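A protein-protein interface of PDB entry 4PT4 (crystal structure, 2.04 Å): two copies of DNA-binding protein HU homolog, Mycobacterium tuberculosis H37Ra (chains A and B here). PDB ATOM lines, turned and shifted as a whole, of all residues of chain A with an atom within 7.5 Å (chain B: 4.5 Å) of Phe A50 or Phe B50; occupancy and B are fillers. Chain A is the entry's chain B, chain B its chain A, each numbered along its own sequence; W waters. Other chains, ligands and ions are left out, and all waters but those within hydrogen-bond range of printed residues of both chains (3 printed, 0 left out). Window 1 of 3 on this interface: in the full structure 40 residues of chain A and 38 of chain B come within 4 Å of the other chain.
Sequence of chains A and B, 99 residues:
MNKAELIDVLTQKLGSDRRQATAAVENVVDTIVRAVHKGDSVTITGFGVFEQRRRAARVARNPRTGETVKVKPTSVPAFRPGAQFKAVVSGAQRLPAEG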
ATOM      1  N   MET A   1      -7.094  17.694  17.978  1.00  0.00           N
ATOM      2  CA  MET A   1      -5.687  17.825  18.434  1.00  0.00           C
ATOM      3  C   MET A   1      -5.229  19.249  18.174  1.00  0.00           C
ATOM      4  O   MET A   1      -5.322  19.712  17.059  1.00  0.00           O
ATOM      5  CB  MET A   1      -4.799  16.851  17.653  1.00  0.00           C
ATOM      6  CG  MET A   1      -3.340  16.965  18.041  1.00  0.00           C
ATOM      7  SD  MET A   1      -2.279  15.810  17.181  1.00  0.00           S
ATOM      8  CE  MET A   1      -2.533  14.289  18.081  1.00  0.00           C
ATOM      9  N   LEU A   6       0.043  18.130  19.313  1.00  0.00           N
ATOM     10  CA  LEU A   6       0.899  17.574  18.262  1.00  0.00           C
ATOM     11  C   LEU A   6       2.387  17.597  18.687  1.00  0.00           C
ATOM     12  O   LEU A   6       3.083  16.618  18.546  1.00  0.00           O
ATOM     13  CB  LEU A   6       0.705  18.325  16.935  1.00  0.00           C
ATOM     14  CG  LEU A   6       1.681  18.048  15.772  1.00  0.00           C
ATOM     15  CD1 LEU A   6       1.456  16.647  15.220  1.00  0.00           C
ATOM     16  CD2 LEU A   6       1.486  19.110  14.696  1.00  0.00           C
ATOM     17  N   VAL A  28       8.986  22.712   9.758  1.00  0.00           N
ATOM     18  CA  VAL A  28       8.327  22.011   8.702  1.00  0.00           C
ATOM     19  C   VAL A  28       7.331  22.971   8.067  1.00  0.00           C
ATOM     20  O   VAL A  28       7.253  23.076   6.862  1.00  0.00           O
ATOM     21  CB  VAL A  28       7.541  20.764   9.146  1.00  0.00           C
ATOM     22  CG1 VAL A  28       6.619  20.365   8.001  1.00  0.00           C
ATOM     23  CG2 VAL A  28       8.484  19.642   9.482  1.00  0.00           C
ATOM     24  N   ILE A  32       7.362  24.469   4.064  1.00  0.00           N
ATOM     25  CA  ILE A  32       6.224  24.294   3.206  1.00  0.00           C
ATOM     26  C   ILE A  32       5.605  25.627   2.724  1.00  0.00           C
ATOM     27  O   ILE A  32       5.396  25.812   1.544  1.00  0.00           O
ATOM     28  CB  ILE A  32       5.156  23.398   3.846  1.00  0.00           C
ATOM     29  CG1 ILE A  32       5.743  21.999   4.080  1.00  0.00           C
ATOM     30  CG2 ILE A  32       3.940  23.325   2.924  1.00  0.00           C
ATOM     31  CD1 ILE A  32       4.815  21.066   4.818  1.00  0.00           C
ATOM     32  N   VAL A  33       5.319  26.520   3.649  1.00  0.00           N
ATOM     33  CA  VAL A  33       4.694  27.783   3.336  1.00  0.00           C
ATOM     34  C   VAL A  33       5.574  28.566   2.315  1.00  0.00           C
ATOM     35  O   VAL A  33       5.091  29.102   1.303  1.00  0.00           O
ATOM     36  CB  VAL A  33       4.515  28.584   4.657  1.00  0.00           C
ATOM     37  CG1 VAL A  33       4.178  30.035   4.365  1.00  0.00           C
ATOM     38  CG2 VAL A  33       3.462  27.956   5.539  1.00  0.00           C
ATOM     39  N   ALA A  35       7.860  27.501   0.251  1.00  0.00           N
ATOM     40  CA  ALA A  35       7.954  26.884  -1.074  1.00  0.00           C
ATOM     41  C   ALA A  35       6.687  27.191  -1.852  1.00  0.00           C
ATOM     42  O   ALA A  35       6.711  27.552  -3.006  1.00  0.00           O
ATOM     43  CB  ALA A  35       8.180  25.377  -0.959  1.00  0.00           C
ATOM     44  N   VAL A  36       5.547  27.052  -1.205  1.00  0.00           N
ATOM     45  CA  VAL A  36       4.302  27.377  -1.851  1.00  0.00           C
ATOM     46  C   VAL A  36       4.316  28.874  -2.199  1.00  0.00           C
ATOM     47  O   VAL A  36       3.825  29.296  -3.234  1.00  0.00           O
ATOM     48  CB  VAL A  36       3.115  27.011  -0.945  1.00  0.00           C
ATOM     49  CG1 VAL A  36       1.835  27.665  -1.433  1.00  0.00           C
ATOM     50  CG2 VAL A  36       2.936  25.492  -0.885  1.00  0.00           C
ATOM     51  N   GLY A  39       5.757  29.674  -5.333  1.00  0.00           N
ATOM     52  CA  GLY A  39       5.018  29.057  -6.414  1.00  0.00           C
ATOM     53  C   GLY A  39       5.387  27.616  -6.655  1.00  0.00           C
ATOM     54  O   GLY A  39       4.814  26.969  -7.532  1.00  0.00           O
ATOM     55  N   ASP A  40       6.324  27.103  -5.875  1.00  0.00           N
ATOM     56  CA  ASP A  40       6.713  25.716  -5.990  1.00  0.00           C
ATOM     57  C   ASP A  40       5.717  24.884  -5.166  1.00  0.00           C
ATOM     58  O   ASP A  40       4.987  25.427  -4.331  1.00  0.00           O
ATOM     59  CB  ASP A  40       8.177  25.520  -5.540  1.00  0.00           C
ATOM     60  CG  ASP A  40       8.871  24.315  -6.226  1.00  0.00           C
ATOM     61  OD1 ASP A  40       8.608  24.033  -7.429  1.00  0.00           O
ATOM     62  OD2 ASP A  40       9.712  23.655  -5.563  1.00  0.00           O
ATOM     63  N   SER A  41       5.648  23.589  -5.458  1.00  0.00           N
ATOM     64  CA  SER A  41       4.805  22.655  -4.743  1.00  0.00           C
ATOM     65  C   SER A  41       5.678  21.772  -3.861  1.00  0.00           C
ATOM     66  O   SER A  41       6.885  21.555  -4.128  1.00  0.00           O
ATOM     67  CB  SER A  41       3.984  21.781  -5.719  1.00  0.00           C
ATOM     68  OG  SER A  41       2.965  22.536  -6.415  1.00  0.00           O
ATOM     69  N   VAL A  42       5.071  21.260  -2.803  1.00  0.00           N
ATOM     70  CA  VAL A  42       5.766  20.386  -1.903  1.00  0.00           C
ATOM     71  C   VAL A  42       5.030  19.076  -1.865  1.00  0.00           C
ATOM     72  O   VAL A  42       3.884  19.016  -1.439  1.00  0.00           O
ATOM     73  CB  VAL A  42       5.859  20.967  -0.502  1.00  0.00           C
ATOM     74  CG1 VAL A  42       6.692  20.038   0.368  1.00  0.00           C
ATOM     75  CG2 VAL A  42       6.481  22.350  -0.551  1.00  0.00           C
ATOM     76  N   THR A  43       5.672  18.023  -2.359  1.00  0.00           N
ATOM     77  CA  THR A  43       5.073  16.694  -2.335  1.00  0.00           C
ATOM     78  C   THR A  43       5.647  15.907  -1.171  1.00  0.00           C
ATOM     79  O   THR A  43       6.852  15.581  -1.130  1.00  0.00           O
ATOM     80  CB  THR A  43       5.302  15.896  -3.629  1.00  0.00           C
ATOM     81  OG1 THR A  43       4.795  16.610  -4.757  1.00  0.00           O
ATOM     82  CG2 THR A  43       4.578  14.529  -3.550  1.00  0.00           C
ATOM     83  N   ILE A  44       4.789  15.602  -0.224  1.00  0.00           N
ATOM     84  CA  ILE A  44       5.174  14.708   0.852  1.00  0.00           C
ATOM     85  C   ILE A  44       4.488  13.390   0.571  1.00  0.00           C
ATOM     86  O   ILE A  44       3.332  13.168   0.934  1.00  0.00           O
ATOM     87  CB  ILE A  44       4.814  15.221   2.264  1.00  0.00           C
ATOM     88  CG1 ILE A  44       5.288  16.672   2.442  1.00  0.00           C
ATOM     89  CG2 ILE A  44       5.434  14.292   3.306  1.00  0.00           C
ATOM     90  CD1 ILE A  44       4.741  17.351   3.687  1.00  0.00           C
ATOM     91  N   PHE A  47       1.420  11.396   2.059  1.00  0.00           N
ATOM     92  CA  PHE A  47       0.618  12.385   2.797  1.00  0.00           C
ATOM     93  C   PHE A  47      -0.211  13.250   1.845  1.00  0.00           C
ATOM     94  O   PHE A  47      -1.442  13.241   1.905  1.00  0.00           O
ATOM     95  CB  PHE A  47       1.547  13.228   3.639  1.00  0.00           C
ATOM     96  CG  PHE A  47       0.863  14.173   4.582  1.00  0.00           C
ATOM     97  CD1 PHE A  47      -0.063  13.725   5.522  1.00  0.00           C
ATOM     98  CD2 PHE A  47       1.246  15.510   4.608  1.00  0.00           C
ATOM     99  CE1 PHE A  47      -0.643  14.618   6.409  1.00  0.00           C
ATOM    100  CE2 PHE A  47       0.696  16.392   5.505  1.00  0.00           C
ATOM    101  CZ  PHE A  47      -0.268  15.949   6.396  1.00  0.00           C
ATOM    102  N   GLY A  48       0.459  13.970   0.947  1.00  0.00           N
ATOM    103  CA  GLY A  48      -0.222  14.813  -0.021  1.00  0.00           C
ATOM    104  C   GLY A  48       0.717  15.849  -0.614  1.00  0.00           C
ATOM    105  O   GLY A  48       1.947  15.770  -0.473  1.00  0.00           O
ATOM    106  N   VAL A  49       0.119  16.822  -1.296  1.00  0.00           N
ATOM    107  CA  VAL A  49       0.857  17.822  -2.051  1.00  0.00           C
ATOM    108  C   VAL A  49       0.283  19.175  -1.662  1.00  0.00           C
ATOM    109  O   VAL A  49      -0.917  19.397  -1.730  1.00  0.00           O
ATOM    110  CB  VAL A  49       0.714  17.615  -3.580  1.00  0.00           C
ATOM    111  CG1 VAL A  49       1.438  18.710  -4.341  1.00  0.00           C
ATOM    112  CG2 VAL A  49       1.233  16.250  -4.017  1.00  0.00           C
ATOM    113  N   PHE A  50       1.153  20.062  -1.226  1.00  0.00           N
ATOM    114  CA  PHE A  50       0.789  21.439  -0.962  1.00  0.00           C
ATOM    115  C   PHE A  50       1.158  22.216  -2.207  1.00  0.00           C
ATOM    116  O   PHE A  50       2.235  22.047  -2.734  1.00  0.00           O
ATOM    117  CB  PHE A  50       1.560  21.981   0.224  1.00  0.00           C
ATOM    118  CG  PHE A  50       1.227  21.317   1.489  1.00  0.00           C
ATOM    119  CD1 PHE A  50       1.920  20.174   1.895  1.00  0.00           C
ATOM    120  CD2 PHE A  50       0.223  21.811   2.305  1.00  0.00           C
ATOM    121  CE1 PHE A  50       1.614  19.552   3.088  1.00  0.00           C
ATOM    122  CE2 PHE A  50      -0.087  21.180   3.499  1.00  0.00           C
ATOM    123  CZ  PHE A  50       0.604  20.046   3.881  1.00  0.00           C
ATOM    124  N   GLU A  51       0.254  23.052  -2.677  1.00  0.00           N
ATOM    125  CA  GLU A  51       0.505  23.827  -3.847  1.00  0.00           C
ATOM    126  C   GLU A  51      -0.121  25.198  -3.726  1.00  0.00           C
ATOM    127  O   GLU A  51      -0.939  25.474  -2.829  1.00  0.00           O
ATOM    128  CB  GLU A  51      -0.016  23.082  -5.079  1.00  0.00           C
ATOM    129  CG  GLU A  51      -1.495  22.778  -5.002  1.00  0.00           C
ATOM    130  CD  GLU A  51      -1.976  21.789  -6.050  1.00  0.00           C
ATOM    131  OE1 GLU A  51      -1.158  21.250  -6.819  1.00  0.00           O
ATOM    132  OE2 GLU A  51      -3.196  21.529  -6.085  1.00  0.00           O
ATOM    133  N   GLN A  52       0.333  26.061  -4.614  1.00  0.00           N
ATOM    134  CA  GLN A  52      -0.226  27.382  -4.793  1.00  0.00           C
ATOM    135  C   GLN A  52      -1.125  27.337  -6.025  1.00  0.00           C
ATOM    136  O   GLN A  52      -0.776  26.714  -7.013  1.00  0.00           O
ATOM    137  CB  GLN A  52       0.894  28.388  -5.025  1.00  0.00           C
ATOM    138  CG  GLN A  52       0.379  29.781  -5.152  1.00  0.00           C
ATOM    139  CD  GLN A  52       1.435  30.762  -5.595  1.00  0.00           C
ATOM    140  OE1 GLN A  52       1.235  31.505  -6.547  1.00  0.00           O
ATOM    141  NE2 GLN A  52       2.545  30.790  -4.898  1.00  0.00           N
ATOM    142  N   PRO A  77      -3.066  28.996  -1.294  1.00  0.00           N
ATOM    143  CA  PRO A  77      -2.468  27.723  -0.975  1.00  0.00           C
ATOM    144  C   PRO A  77      -3.506  26.628  -1.041  1.00  0.00           C
ATOM    145  O   PRO A  77      -4.680  26.883  -0.801  1.00  0.00           O
ATOM    146  CB  PRO A  77      -2.000  27.905   0.469  1.00  0.00           C
ATOM    147  CG  PRO A  77      -2.906  28.908   1.028  1.00  0.00           C
ATOM    148  CD  PRO A  77      -3.354  29.784  -0.090  1.00  0.00           C
ATOM    149  N   ALA A  78      -3.064  25.416  -1.329  1.00  0.00           N
ATOM    150  CA  ALA A  78      -3.964  24.266  -1.345  1.00  0.00           C
ATOM    151  C   ALA A  78      -3.223  22.989  -1.018  1.00  0.00           C
ATOM    152  O   ALA A  78      -2.020  22.899  -1.265  1.00  0.00           O
ATOM    153  CB  ALA A  78      -4.560  24.136  -2.741  1.00  0.00           C
ATOM    154  N   PHE A  79      -3.950  21.991  -0.514  1.00  0.00           N
ATOM    155  CA  PHE A  79      -3.382  20.686  -0.225  1.00  0.00           C
ATOM    156  C   PHE A  79      -4.253  19.636  -0.844  1.00  0.00           C
ATOM    157  O   PHE A  79      -5.454  19.633  -0.592  1.00  0.00           O
ATOM    158  CB  PHE A  79      -3.285  20.490   1.277  1.00  0.00           C
ATOM    159  CG  PHE A  79      -2.945  19.087   1.718  1.00  0.00           C
ATOM    160  CD1 PHE A  79      -1.616  18.659   1.789  1.00  0.00           C
ATOM    161  CD2 PHE A  79      -3.941  18.217   2.132  1.00  0.00           C
ATOM    162  CE1 PHE A  79      -1.290  17.381   2.211  1.00  0.00           C
ATOM    163  CE2 PHE A  79      -3.603  16.930   2.583  1.00  0.00           C
ATOM    164  CZ  PHE A  79      -2.281  16.525   2.611  1.00  0.00           C
ATOM    165  N   ARG A  80      -3.635  18.772  -1.664  1.00  0.00           N
ATOM    166  CA  ARG A  80      -4.269  17.619  -2.260  1.00  0.00           C
ATOM    167  C   ARG A  80      -3.833  16.408  -1.481  1.00  0.00           C
ATOM    168  O   ARG A  80      -2.678  16.025  -1.546  1.00  0.00           O
ATOM    169  CB  ARG A  80      -3.830  17.423  -3.728  1.00  0.00           C
ATOM    170  CG  ARG A  80      -4.716  18.149  -4.713  1.00  0.00           C
ATOM    171  CD  ARG A  80      -4.426  17.772  -6.161  1.00  0.00           C
ATOM    172  NE  ARG A  80      -3.203  18.434  -6.592  1.00  0.00           N
ATOM    173  CZ  ARG A  80      -2.047  17.827  -6.739  1.00  0.00           C
ATOM    174  NH1 ARG A  80      -1.000  18.524  -7.111  1.00  0.00           N
ATOM    175  NH2 ARG A  80      -1.942  16.532  -6.519  1.00  0.00           N
ATOM    176  N   PRO A  81      -4.768  15.783  -0.760  1.00  0.00           N
ATOM    177  CA  PRO A  81      -4.508  14.573  -0.005  1.00  0.00           C
ATOM    178  C   PRO A  81      -3.981  13.474  -0.874  1.00  0.00           C
ATOM    179  O   PRO A  81      -4.492  13.244  -1.966  1.00  0.00           O
ATOM    180  CB  PRO A  81      -5.894  14.196   0.516  1.00  0.00           C
ATOM    181  CG  PRO A  81      -6.605  15.494   0.602  1.00  0.00           C
ATOM    182  CD  PRO A  81      -6.163  16.234  -0.595  1.00  0.00           C
ATOM    183  N   PHE A  85      -3.014   8.558   2.250  1.00  0.00           N
ATOM    184  CA  PHE A  85      -3.773   9.252   3.264  1.00  0.00           C
ATOM    185  C   PHE A  85      -5.284   9.001   3.027  1.00  0.00           C
ATOM    186  O   PHE A  85      -6.025   8.755   3.988  1.00  0.00           O
ATOM    187  CB  PHE A  85      -3.467  10.755   3.194  1.00  0.00           C
ATOM    188  CG  PHE A  85      -3.928  11.551   4.392  1.00  0.00           C
ATOM    189  CD1 PHE A  85      -4.705  10.992   5.410  1.00  0.00           C
ATOM    190  CD2 PHE A  85      -3.597  12.889   4.481  1.00  0.00           C
ATOM    191  CE1 PHE A  85      -5.113  11.752   6.485  1.00  0.00           C
ATOM    192  CE2 PHE A  85      -4.014  13.657   5.545  1.00  0.00           C
ATOM    193  CZ  PHE A  85      -4.762  13.093   6.549  1.00  0.00           C
ATOM    194  N   ILE B  32      -0.462  13.327  12.338  1.00  0.00           N
ATOM    195  CA  ILE B  32      -1.573  13.979  11.688  1.00  0.00           C
ATOM    196  C   ILE B  32      -2.541  12.945  11.128  1.00  0.00           C
ATOM    197  O   ILE B  32      -3.756  13.000  11.379  1.00  0.00           O
ATOM    198  CB  ILE B  32      -1.127  14.974  10.597  1.00  0.00           C
ATOM    199  CG1 ILE B  32      -0.342  16.141  11.246  1.00  0.00           C
ATOM    200  CG2 ILE B  32      -2.343  15.586   9.928  1.00  0.00           C
ATOM    201  CD1 ILE B  32       0.350  17.093  10.285  1.00  0.00           C
ATOM    202  N   VAL B  36      -6.586  12.274  12.259  1.00  0.00           N
ATOM    203  CA  VAL B  36      -7.650  12.439  11.274  1.00  0.00           C
ATOM    204  C   VAL B  36      -8.367  11.096  11.115  1.00  0.00           C
ATOM    205  O   VAL B  36      -9.562  11.026  11.194  1.00  0.00           O
ATOM    206  CB  VAL B  36      -7.097  13.004   9.946  1.00  0.00           C
ATOM    207  CG1 VAL B  36      -8.144  12.989   8.823  1.00  0.00           C
ATOM    208  CG2 VAL B  36      -6.594  14.445  10.141  1.00  0.00           C
ATOM    209  N   ASP B  40     -10.458  12.987  14.522  1.00  0.00           N
ATOM    210  CA  ASP B  40     -10.057  14.221  15.174  1.00  0.00           C
ATOM    211  C   ASP B  40      -9.556  15.213  14.102  1.00  0.00           C
ATOM    212  O   ASP B  40      -9.173  14.817  12.998  1.00  0.00           O
ATOM    213  CB  ASP B  40      -9.034  13.944  16.275  1.00  0.00           C
ATOM    214  CG  ASP B  40      -9.648  13.188  17.460  1.00  0.00           C
ATOM    215  OD1 ASP B  40     -10.835  13.419  17.799  1.00  0.00           O
ATOM    216  OD2 ASP B  40      -8.953  12.348  18.056  1.00  0.00           O
ATOM    217  N   SER B  41      -9.647  16.495  14.396  1.00  0.00           N
ATOM    218  CA  SER B  41      -9.039  17.507  13.569  1.00  0.00           C
ATOM    219  C   SER B  41      -7.692  17.867  14.160  1.00  0.00           C
ATOM    220  O   SER B  41      -7.471  17.722  15.376  1.00  0.00           O
ATOM    221  CB  SER B  41      -9.945  18.746  13.470  1.00  0.00           C
ATOM    222  OG  SER B  41     -10.003  19.447  14.710  1.00  0.00           O
ATOM    223  N   VAL B  42      -6.780  18.334  13.304  1.00  0.00           N
ATOM    224  CA  VAL B  42      -5.497  18.786  13.773  1.00  0.00           C
ATOM    225  C   VAL B  42      -5.355  20.227  13.352  1.00  0.00           C
ATOM    226  O   VAL B  42      -5.278  20.501  12.168  1.00  0.00           O
ATOM    227  CB  VAL B  42      -4.328  17.976  13.199  1.00  0.00           C
ATOM    228  CG1 VAL B  42      -3.025  18.521  13.779  1.00  0.00           C
ATOM    229  CG2 VAL B  42      -4.472  16.490  13.510  1.00  0.00           C
ATOM    230  N   ILE B  44      -2.848  23.183  13.183  1.00  0.00           N
ATOM    231  CA  ILE B  44      -1.488  23.686  13.302  1.00  0.00           C
ATOM    232  C   ILE B  44      -1.651  25.170  13.097  1.00  0.00           C
ATOM    233  O   ILE B  44      -1.789  25.656  11.963  1.00  0.00           O
ATOM    234  CB  ILE B  44      -0.507  23.086  12.295  1.00  0.00           C
ATOM    235  CG1 ILE B  44      -0.598  21.554  12.357  1.00  0.00           C
ATOM    236  CG2 ILE B  44       0.895  23.625  12.588  1.00  0.00           C
ATOM    237  CD1 ILE B  44       0.354  20.822  11.452  1.00  0.00           C
ATOM    238  N   PHE B  47      -0.940  27.630  10.092  1.00  0.00           N
ATOM    239  CA  PHE B  47      -0.698  26.845   8.869  1.00  0.00           C
ATOM    240  C   PHE B  47      -2.036  26.415   8.299  1.00  0.00           C
ATOM    241  O   PHE B  47      -2.363  26.745   7.156  1.00  0.00           O
ATOM    242  CB  PHE B  47       0.171  25.649   9.235  1.00  0.00           C
ATOM    243  CG  PHE B  47       0.595  24.788   8.082  1.00  0.00           C
ATOM    244  CD1 PHE B  47       1.271  25.317   6.989  1.00  0.00           C
ATOM    245  CD2 PHE B  47       0.387  23.417   8.132  1.00  0.00           C
ATOM    246  CE1 PHE B  47       1.691  24.501   5.963  1.00  0.00           C
ATOM    247  CE2 PHE B  47       0.838  22.600   7.132  1.00  0.00           C
ATOM    248  CZ  PHE B  47       1.466  23.144   6.035  1.00  0.00           C
ATOM    249  N   GLY B  48      -2.810  25.689   9.103  1.00  0.00           N
ATOM    250  CA  GLY B  48      -4.111  25.179   8.670  1.00  0.00           C
ATOM    251  C   GLY B  48      -4.630  24.058   9.559  1.00  0.00           C
ATOM    252  O   GLY B  48      -4.006  23.671  10.569  1.00  0.00           O
ATOM    253  N   VAL B  49      -5.792  23.549   9.187  1.00  0.00           N
ATOM    254  CA  VAL B  49      -6.485  22.488   9.950  1.00  0.00           C
ATOM    255  C   VAL B  49      -6.672  21.305   9.050  1.00  0.00           C
ATOM    256  O   VAL B  49      -7.238  21.418   7.970  1.00  0.00           O
ATOM    257  CB  VAL B  49      -7.886  22.930  10.417  1.00  0.00           C
ATOM    258  CG1 VAL B  49      -8.598  21.811  11.165  1.00  0.00           C
ATOM    259  CG2 VAL B  49      -7.795  24.188  11.256  1.00  0.00           C
ATOM    260  N   PHE B  50      -6.209  20.161   9.517  1.00  0.00           N
ATOM    261  CA  PHE B  50      -6.420  18.909   8.831  1.00  0.00           C
ATOM    262  C   PHE B  50      -7.638  18.304   9.485  1.00  0.00           C
ATOM    263  O   PHE B  50      -7.763  18.326  10.699  1.00  0.00           O
ATOM    264  CB  PHE B  50      -5.216  17.979   8.996  1.00  0.00           C
ATOM    265  CG  PHE B  50      -4.003  18.444   8.274  1.00  0.00           C
ATOM    266  CD1 PHE B  50      -3.763  18.054   6.953  1.00  0.00           C
ATOM    267  CD2 PHE B  50      -3.076  19.255   8.906  1.00  0.00           C
ATOM    268  CE1 PHE B  50      -2.641  18.495   6.283  1.00  0.00           C
ATOM    269  CE2 PHE B  50      -1.934  19.683   8.241  1.00  0.00           C
ATOM    270  CZ  PHE B  50      -1.729  19.310   6.939  1.00  0.00           C
ATOM    271  N   GLU B  51      -8.564  17.792   8.694  1.00  0.00           N
ATOM    272  CA  GLU B  51      -9.692  17.080   9.284  1.00  0.00           C
ATOM    273  C   GLU B  51     -10.186  15.950   8.392  1.00  0.00           C
ATOM    274  O   GLU B  51      -9.748  15.799   7.242  1.00  0.00           O
ATOM    275  CB  GLU B  51     -10.814  18.064   9.597  1.00  0.00           C
ATOM    276  CG  GLU B  51     -11.136  19.024   8.451  1.00  0.00           C
ATOM    277  CD  GLU B  51     -12.331  19.929   8.739  1.00  0.00           C
ATOM    278  OE1 GLU B  51     -12.874  19.904   9.856  1.00  0.00           O
ATOM    279  OE2 GLU B  51     -12.743  20.664   7.833  1.00  0.00           O
ATOM    280  N   ALA B  78      -8.949  16.323   4.543  1.00  0.00           N
ATOM    281  CA  ALA B  78      -8.980  17.664   3.991  1.00  0.00           C
ATOM    282  C   ALA B  78      -8.098  18.569   4.789  1.00  0.00           C
ATOM    283  O   ALA B  78      -7.914  18.339   5.968  1.00  0.00           O
ATOM    284  CB  ALA B  78     -10.413  18.196   4.039  1.00  0.00           C
ATOM    285  N   PHE B  79      -7.604  19.629   4.161  1.00  0.00           N
ATOM    286  CA  PHE B  79      -6.818  20.649   4.851  1.00  0.00           C
ATOM    287  C   PHE B  79      -7.404  21.991   4.499  1.00  0.00           C
ATOM    288  O   PHE B  79      -7.518  22.297   3.333  1.00  0.00           O
ATOM    289  CB  PHE B  79      -5.352  20.573   4.363  1.00  0.00           C
ATOM    290  CG  PHE B  79      -4.442  21.707   4.840  1.00  0.00           C
ATOM    291  CD1 PHE B  79      -3.919  21.711   6.117  1.00  0.00           C
ATOM    292  CD2 PHE B  79      -4.069  22.742   3.970  1.00  0.00           C
ATOM    293  CE1 PHE B  79      -3.081  22.729   6.550  1.00  0.00           C
ATOM    294  CE2 PHE B  79      -3.209  23.762   4.388  1.00  0.00           C
ATOM    295  CZ  PHE B  79      -2.731  23.764   5.689  1.00  0.00           C
HETATM  296  O   HOH W   1      -6.736  22.541   0.534  1.00  0.00           O
HETATM  297  O   HOH W   2      -7.740  19.538   1.218  1.00  0.00           O
HETATM  298  O   HOH W   3      -8.386  21.154  16.415  1.00  0.00           O
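Water W3 bridges OG of Ser B41 and O of Met A1. Water W1 lies within hydrogen-bond range of O of Phe B79 and N of Phe A79. Water W2 bridges O of Phe A79 and N of Phe B79.
Of the 25 printed residues of chain A, 7 touch a printed residue of chain B. Hydrophobic or aromatic side chains of chain A within 4 Å of the printed part of chain B: Met A1, Leu A6, Ile A32, Val A33, Phe A47, Phe A50 and Phe A79. Hydrophobic or aromatic side chains of chain B within 4 Å of the printed part of chain A: Ile B44, Phe B47, Phe B50 and Phe B79. Among the printed residues, 9 pairs touch across the chains. Among the printed residues, no Asp or Glu carboxylate lies within 4 Å of a Lys or Arg side-chain nitrogen of the other chain.
The backbone carbonyl oxygen of Ser B41 sits at hydrogen-bond distance from the backbone NH of Met A1, 2.6 Å away.
Ile A32 touches Phe B47, but with the chains exchanged Phe A47 does not touch Ile B32 (4.03 Å). Phe A47 touches Phe B50, and with the chains exchanged Phe A50 touches Phe B47. Phe B50 touches its own counterpart, Phe A50. Phe A79 touches its own counterpart, Phe B79. Of the 9 pairs that touch across the chains among the printed residues, 4 have their exchanged pair printed and touching as well.
Of chain B, only Phe B47 and Phe B50 come within 4 Å of Phe A50. Phe B50 touches just these residues of chain A: Phe A47 and Phe A50. Printed residues of chain A within 4 Å of Val B42: Met A1. Of the printed residues of chain B, Met A1 touches Ser B41 (2.6 Å) and Val B42 (3.4 Å). Of the printed residues of chain B, Ile A32 touches Phe B47 (3.96 Å). Printed residues of chain A within 4 Å of Phe B79: Phe A79. Printed residues of chain B within 4 Å of Val A33: Phe B47 (3.7 Å). The nearest residue of chain A that does not touch Phe B50 is Phe A79 (4.1 Å).
Among the printed residues, pairs that only touch across the chains: Met A1 with Val B42, Leu A6 with Ile B44, Ile A32 with Phe B47, Val A33 with Phe B47, Phe A47 with Phe B50, Phe A50 with Phe B47, Phe A50 with Phe B50 and Phe A79 with Phe B79.
O of Val A42 lies within hydrogen-bond range of N of Phe A50 (2.9 Å). The backbone NH (N) of Val B42 is in hydrogen-bond range of the backbone carbonyl oxygen (O) of Phe B50, 2.8 Å away.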
